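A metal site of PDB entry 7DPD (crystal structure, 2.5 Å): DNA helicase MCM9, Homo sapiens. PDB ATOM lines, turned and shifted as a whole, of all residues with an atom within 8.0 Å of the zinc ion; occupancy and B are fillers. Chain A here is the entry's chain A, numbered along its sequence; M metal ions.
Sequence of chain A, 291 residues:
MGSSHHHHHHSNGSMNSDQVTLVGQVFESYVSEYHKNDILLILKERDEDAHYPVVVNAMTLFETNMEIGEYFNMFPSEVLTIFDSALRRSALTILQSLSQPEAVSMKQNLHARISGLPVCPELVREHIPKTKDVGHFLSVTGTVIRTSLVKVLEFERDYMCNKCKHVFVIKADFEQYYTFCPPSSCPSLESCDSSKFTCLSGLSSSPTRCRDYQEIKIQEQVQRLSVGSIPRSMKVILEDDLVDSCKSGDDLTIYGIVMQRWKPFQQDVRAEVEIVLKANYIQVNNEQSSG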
ATOM      1  N   MET A 160     -22.285 -21.392  29.103  1.00  0.00           N
ATOM      2  CA  MET A 160     -22.557 -22.261  30.236  1.00  0.00           C
ATOM      3  C   MET A 160     -24.068 -22.448  30.349  1.00  0.00           C
ATOM      4  O   MET A 160     -24.854 -21.599  29.909  1.00  0.00           O
ATOM      5  CB  MET A 160     -21.975 -21.706  31.538  1.00  0.00           C
ATOM      6  CG  MET A 160     -22.805 -20.622  32.187  1.00  0.00           C
ATOM      7  SD  MET A 160     -22.119 -20.031  33.757  1.00  0.00           S
ATOM      8  CE  MET A 160     -23.419 -18.925  34.300  1.00  0.00           C
ATOM      9  N   CYS A 161     -24.457 -23.561  30.954  1.00  0.00           N
ATOM     10  CA  CYS A 161     -25.859 -23.861  31.180  1.00  0.00           C
ATOM     11  C   CYS A 161     -26.312 -23.285  32.514  1.00  0.00           C
ATOM     12  O   CYS A 161     -25.600 -23.391  33.519  1.00  0.00           O
ATOM     13  CB  CYS A 161     -26.109 -25.374  31.150  1.00  0.00           C
ATOM     14  SG  CYS A 161     -27.849 -25.854  31.081  1.00  0.00           S
ATOM     15  N   ASN A 162     -27.489 -22.665  32.515  1.00  0.00           N
ATOM     16  CA  ASN A 162     -28.009 -22.051  33.734  1.00  0.00           C
ATOM     17  C   ASN A 162     -28.460 -23.083  34.766  1.00  0.00           C
ATOM     18  O   ASN A 162     -28.586 -22.749  35.948  1.00  0.00           O
ATOM     19  CB  ASN A 162     -29.163 -21.108  33.401  1.00  0.00           C
ATOM     20  CG  ASN A 162     -28.695 -19.853  32.695  1.00  0.00           C
ATOM     21  OD1 ASN A 162     -27.570 -19.785  32.200  1.00  0.00           O
ATOM     22  ND2 ASN A 162     -29.565 -18.846  32.659  1.00  0.00           N
ATOM     23  N   LYS A 163     -28.715 -24.318  34.349  1.00  0.00           N
ATOM     24  CA  LYS A 163     -29.204 -25.351  35.257  1.00  0.00           C
ATOM     25  C   LYS A 163     -28.142 -26.347  35.673  1.00  0.00           C
ATOM     26  O   LYS A 163     -28.202 -26.856  36.796  1.00  0.00           O
ATOM     27  CB  LYS A 163     -30.381 -26.108  34.625  1.00  0.00           C
ATOM     28  CG  LYS A 163     -31.612 -25.247  34.371  1.00  0.00           C
ATOM     29  CD  LYS A 163     -32.783 -26.083  33.905  1.00  0.00           C
ATOM     30  CE  LYS A 163     -34.021 -25.231  33.670  1.00  0.00           C
ATOM     31  NZ  LYS A 163     -35.176 -26.047  33.189  1.00  0.00           N
ATOM     32  N   CYS A 164     -27.165 -26.647  34.815  1.00  0.00           N
ATOM     33  CA  CYS A 164     -26.136 -27.623  35.120  1.00  0.00           C
ATOM     34  C   CYS A 164     -24.738 -27.050  35.231  1.00  0.00           C
ATOM     35  O   CYS A 164     -23.817 -27.779  35.625  1.00  0.00           O
ATOM     36  CB  CYS A 164     -26.137 -28.745  34.069  1.00  0.00           C
ATOM     37  SG  CYS A 164     -25.893 -28.207  32.350  1.00  0.00           S
ATOM     38  N   LYS A 165     -24.539 -25.766  34.889  1.00  0.00           N
ATOM     39  CA  LYS A 165     -23.220 -25.113  34.956  1.00  0.00           C
ATOM     40  C   LYS A 165     -22.206 -25.823  34.069  1.00  0.00           C
ATOM     41  O   LYS A 165     -21.013 -25.889  34.384  1.00  0.00           O
ATOM     42  CB  LYS A 165     -22.719 -25.019  36.399  1.00  0.00           C
ATOM     43  CG  LYS A 165     -23.539 -24.118  37.316  1.00  0.00           C
ATOM     44  CD  LYS A 165     -24.687 -24.872  37.981  1.00  0.00           C
ATOM     45  CE  LYS A 165     -25.476 -23.988  38.932  1.00  0.00           C
ATOM     46  NZ  LYS A 165     -26.554 -24.733  39.636  1.00  0.00           N
ATOM     47  N   HIS A 166     -22.676 -26.367  32.942  1.00  0.00           N
ATOM     48  CA  HIS A 166     -21.807 -27.063  32.008  1.00  0.00           C
ATOM     49  C   HIS A 166     -21.260 -26.072  30.994  1.00  0.00           C
ATOM     50  O   HIS A 166     -22.030 -25.420  30.275  1.00  0.00           O
ATOM     51  CB  HIS A 166     -22.566 -28.200  31.307  1.00  0.00           C
ATOM     52  CG  HIS A 166     -21.785 -28.881  30.239  1.00  0.00           C
ATOM     53  ND1 HIS A 166     -22.226 -28.961  28.938  1.00  0.00           N
ATOM     54  CD2 HIS A 166     -20.579 -29.497  30.271  1.00  0.00           C
ATOM     55  CE1 HIS A 166     -21.326 -29.621  28.210  1.00  0.00           C
ATOM     56  NE2 HIS A 166     -20.319 -29.955  29.007  1.00  0.00           N
ATOM     57  N   PHE A 168     -19.732 -25.262  27.631  1.00  0.00           N
ATOM     58  CA  PHE A 168     -19.601 -25.778  26.273  1.00  0.00           C
ATOM     59  C   PHE A 168     -19.157 -24.660  25.344  1.00  0.00           C
ATOM     60  O   PHE A 168     -18.980 -23.512  25.763  1.00  0.00           O
ATOM     61  CB  PHE A 168     -20.902 -26.426  25.782  1.00  0.00           C
ATOM     62  CG  PHE A 168     -22.053 -25.468  25.676  1.00  0.00           C
ATOM     63  CD1 PHE A 168     -22.821 -25.154  26.792  1.00  0.00           C
ATOM     64  CD2 PHE A 168     -22.379 -24.888  24.470  1.00  0.00           C
ATOM     65  CE1 PHE A 168     -23.883 -24.278  26.703  1.00  0.00           C
ATOM     66  CE2 PHE A 168     -23.443 -24.003  24.358  1.00  0.00           C
ATOM     67  CZ  PHE A 168     -24.192 -23.698  25.482  1.00  0.00           C
ATOM     68  N   SER A 185     -29.956 -25.405  23.049  1.00  0.00           N
ATOM     69  CA  SER A 185     -29.967 -26.775  23.513  1.00  0.00           C
ATOM     70  C   SER A 185     -28.681 -27.046  24.271  1.00  0.00           C
ATOM     71  O   SER A 185     -27.589 -26.729  23.789  1.00  0.00           O
ATOM     72  CB  SER A 185     -30.110 -27.765  22.347  1.00  0.00           C
ATOM     73  OG  SER A 185     -31.235 -27.451  21.556  1.00  0.00           O
ATOM     74  N   CYS A 186     -28.805 -27.626  25.467  1.00  0.00           N
ATOM     75  CA  CYS A 186     -27.635 -27.894  26.296  1.00  0.00           C
ATOM     76  C   CYS A 186     -26.929 -29.159  25.818  1.00  0.00           C
ATOM     77  O   CYS A 186     -27.539 -30.236  25.858  1.00  0.00           O
ATOM     78  CB  CYS A 186     -28.037 -28.029  27.757  1.00  0.00           C
ATOM     79  SG  CYS A 186     -26.642 -28.186  28.912  1.00  0.00           S
ATOM     80  N   PRO A 187     -25.676 -29.076  25.376  1.00  0.00           N
ATOM     81  CA  PRO A 187     -24.981 -30.272  24.880  1.00  0.00           C
ATOM     82  C   PRO A 187     -24.278 -31.046  25.987  1.00  0.00           C
ATOM     83  O   PRO A 187     -23.242 -31.664  25.744  1.00  0.00           O
ATOM     84  CB  PRO A 187     -23.989 -29.704  23.876  1.00  0.00           C
ATOM     85  CG  PRO A 187     -23.629 -28.379  24.463  1.00  0.00           C
ATOM     86  CD  PRO A 187     -24.876 -27.862  25.151  1.00  0.00           C
ATOM     87  N   SER A 188     -24.818 -30.998  27.202  1.00  0.00           N
ATOM     88  CA  SER A 188     -24.209 -31.720  28.312  1.00  0.00           C
ATOM     89  C   SER A 188     -24.469 -33.220  28.170  1.00  0.00           C
ATOM     90  O   SER A 188     -25.315 -33.666  27.383  1.00  0.00           O
ATOM     91  CB  SER A 188     -24.751 -31.212  29.644  1.00  0.00           C
ATOM     92  OG  SER A 188     -26.163 -31.372  29.721  1.00  0.00           O
ATOM     93  N   LEU A 189     -23.715 -34.011  28.941  1.00  0.00           N
ATOM     94  CA  LEU A 189     -23.898 -35.457  28.915  1.00  0.00           C
ATOM     95  C   LEU A 189     -25.268 -35.857  29.437  1.00  0.00           C
ATOM     96  O   LEU A 189     -25.809 -36.896  29.028  1.00  0.00           O
ATOM     97  CB  LEU A 189     -22.793 -36.144  29.729  1.00  0.00           C
ATOM     98  CG  LEU A 189     -22.835 -36.091  31.266  1.00  0.00           C
ATOM     99  CD1 LEU A 189     -21.910 -37.160  31.854  1.00  0.00           C
ATOM    100  CD2 LEU A 189     -22.460 -34.717  31.803  1.00  0.00           C
ATOM    101  N   GLU A 190     -25.857 -35.059  30.321  1.00  0.00           N
ATOM    102  CA  GLU A 190     -27.200 -35.297  30.839  1.00  0.00           C
ATOM    103  C   GLU A 190     -28.168 -34.360  30.128  1.00  0.00           C
ATOM    104  O   GLU A 190     -27.929 -33.147  30.053  1.00  0.00           O
ATOM    105  CB  GLU A 190     -27.239 -35.075  32.350  1.00  0.00           C
ATOM    106  CG  GLU A 190     -26.283 -35.958  33.131  1.00  0.00           C
ATOM    107  CD  GLU A 190     -26.298 -35.685  34.619  1.00  0.00           C
ATOM    108  OE1 GLU A 190     -27.020 -34.757  35.045  1.00  0.00           O
ATOM    109  OE2 GLU A 190     -25.596 -36.401  35.366  1.00  0.00           O
ATOM    110  N   SER A 191     -29.249 -34.921  29.605  1.00  0.00           N
ATOM    111  CA  SER A 191     -30.202 -34.160  28.797  1.00  0.00           C
ATOM    112  C   SER A 191     -30.841 -33.040  29.609  1.00  0.00           C
ATOM    113  O   SER A 191     -31.740 -33.289  30.427  1.00  0.00           O
ATOM    114  CB  SER A 191     -31.274 -35.085  28.223  1.00  0.00           C
ATOM    115  OG  SER A 191     -32.196 -34.361  27.429  1.00  0.00           O
ATOM    116  N   CYS A 192     -30.394 -31.807  29.391  1.00  0.00           N
ATOM    117  CA  CYS A 192     -30.947 -30.637  30.053  1.00  0.00           C
ATOM    118  C   CYS A 192     -31.943 -29.948  29.132  1.00  0.00           C
ATOM    119  O   CYS A 192     -31.611 -29.648  27.985  1.00  0.00           O
ATOM    120  CB  CYS A 192     -29.843 -29.660  30.456  1.00  0.00           C
ATOM    121  SG  CYS A 192     -28.581 -30.314  31.570  1.00  0.00           S
ATOM    122  N   ASP A 193     -33.142 -29.710  29.642  1.00  0.00           N
ATOM    123  CA  ASP A 193     -34.147 -28.949  28.911  1.00  0.00           C
ATOM    124  C   ASP A 193     -33.906 -27.445  28.991  1.00  0.00           C
ATOM    125  O   ASP A 193     -34.778 -26.673  28.572  1.00  0.00           O
ATOM    126  CB  ASP A 193     -35.545 -29.282  29.430  1.00  0.00           C
ATOM    127  CG  ASP A 193     -35.850 -30.761  29.366  1.00  0.00           C
ATOM    128  OD1 ASP A 193     -35.303 -31.442  28.473  1.00  0.00           O
ATOM    129  OD2 ASP A 193     -36.637 -31.250  30.215  1.00  0.00           O
ATOM    130  N   SER A 194     -32.754 -27.029  29.513  1.00  0.00           N
ATOM    131  CA  SER A 194     -32.471 -25.615  29.678  1.00  0.00           C
ATOM    132  C   SER A 194     -32.162 -24.968  28.328  1.00  0.00           C
ATOM    133  O   SER A 194     -31.322 -25.464  27.571  1.00  0.00           O
ATOM    134  CB  SER A 194     -31.298 -25.422  30.637  1.00  0.00           C
ATOM    135  OG  SER A 194     -30.859 -24.075  30.650  1.00  0.00           O
ATOM    136  N   SER A 195     -32.853 -23.870  28.040  1.00  0.00           N
ATOM    137  CA  SER A 195     -32.561 -23.052  26.873  1.00  0.00           C
ATOM    138  C   SER A 195     -31.903 -21.734  27.236  1.00  0.00           C
ATOM    139  O   SER A 195     -31.568 -20.946  26.347  1.00  0.00           O
ATOM    140  CB  SER A 195     -33.842 -22.783  26.074  1.00  0.00           C
ATOM    141  OG  SER A 195     -34.802 -22.104  26.864  1.00  0.00           O
ATOM    142  N   LYS A 196     -31.708 -21.466  28.529  1.00  0.00           N
ATOM    143  CA  LYS A 196     -31.096 -20.235  29.005  1.00  0.00           C
ATOM    144  C   LYS A 196     -29.602 -20.463  29.209  1.00  0.00           C
ATOM    145  O   LYS A 196     -29.205 -21.270  30.062  1.00  0.00           O
ATOM    146  CB  LYS A 196     -31.751 -19.759  30.302  1.00  0.00           C
ATOM    147  CG  LYS A 196     -32.902 -18.777  30.110  1.00  0.00           C
ATOM    148  CD  LYS A 196     -34.068 -19.399  29.360  1.00  0.00           C
ATOM    149  CE  LYS A 196     -35.192 -18.385  29.145  1.00  0.00           C
ATOM    150  NZ  LYS A 196     -36.308 -18.957  28.338  1.00  0.00           N
ATOM    151  N   PHE A 197     -28.783 -19.755  28.433  1.00  0.00           N
ATOM    152  CA  PHE A 197     -27.336 -19.842  28.527  1.00  0.00           C
ATOM    153  C   PHE A 197     -26.746 -18.446  28.634  1.00  0.00           C
ATOM    154  O   PHE A 197     -27.382 -17.449  28.262  1.00  0.00           O
ATOM    155  CB  PHE A 197     -26.739 -20.580  27.311  1.00  0.00           C
ATOM    156  CG  PHE A 197     -27.350 -21.927  27.054  1.00  0.00           C
ATOM    157  CD1 PHE A 197     -27.518 -22.832  28.100  1.00  0.00           C
ATOM    158  CD2 PHE A 197     -27.747 -22.293  25.779  1.00  0.00           C
ATOM    159  CE1 PHE A 197     -28.087 -24.074  27.869  1.00  0.00           C
ATOM    160  CE2 PHE A 197     -28.316 -23.535  25.548  1.00  0.00           C
ATOM    161  CZ  PHE A 197     -28.472 -24.429  26.588  1.00  0.00           C
HETATM  162 ZN    ZN M   1     -27.760 -28.166  30.973  1.00  0.00          ZN
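SG of Cys 161 binds the zinc ion (2.3 Å). The side-chain sulfur (SG) of Cys 164 is bound to the zinc ion (2.3 Å). The zinc ion is bound by SG of Cys 186, at 2.3 Å. The zinc ion is bound by SG of Cys 192 (2.4 Å). The zinc ion has four donor atoms within binding distance.
OG of Ser 194 lies close to SG of Cys 161 (3.5 Å). N of Lys 163 sits close to SG of Cys 161 (3.7 Å). O of His 166 lies within hydrogen-bond range of N of Cys 161, 3.1 Å away. SG of Cys 164 lies close to N of His 166, 3.8 Å away. OG of Ser 188 lies close to SG of Cys 186. SG of Cys 192 sits close to OG of Ser 188 (3.2 Å). The side-chain sulfur (SG) of Cys 192 lies close to the backbone carbonyl oxygen (O) of Glu 190 (3.3 Å). OG of Ser 188 is in hydrogen-bond range of O of Glu 190 (2.5 Å).
Ser 188 touches the zinc ion (OG to ZN, 3.8 Å). Within 4 Å of the zinc ion: Cys 161, Cys 164, Cys 186, Ser 188 and Cys 192. The nearest printed residue that does not touch the zinc ion is Ser 194 (4.5 Å).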
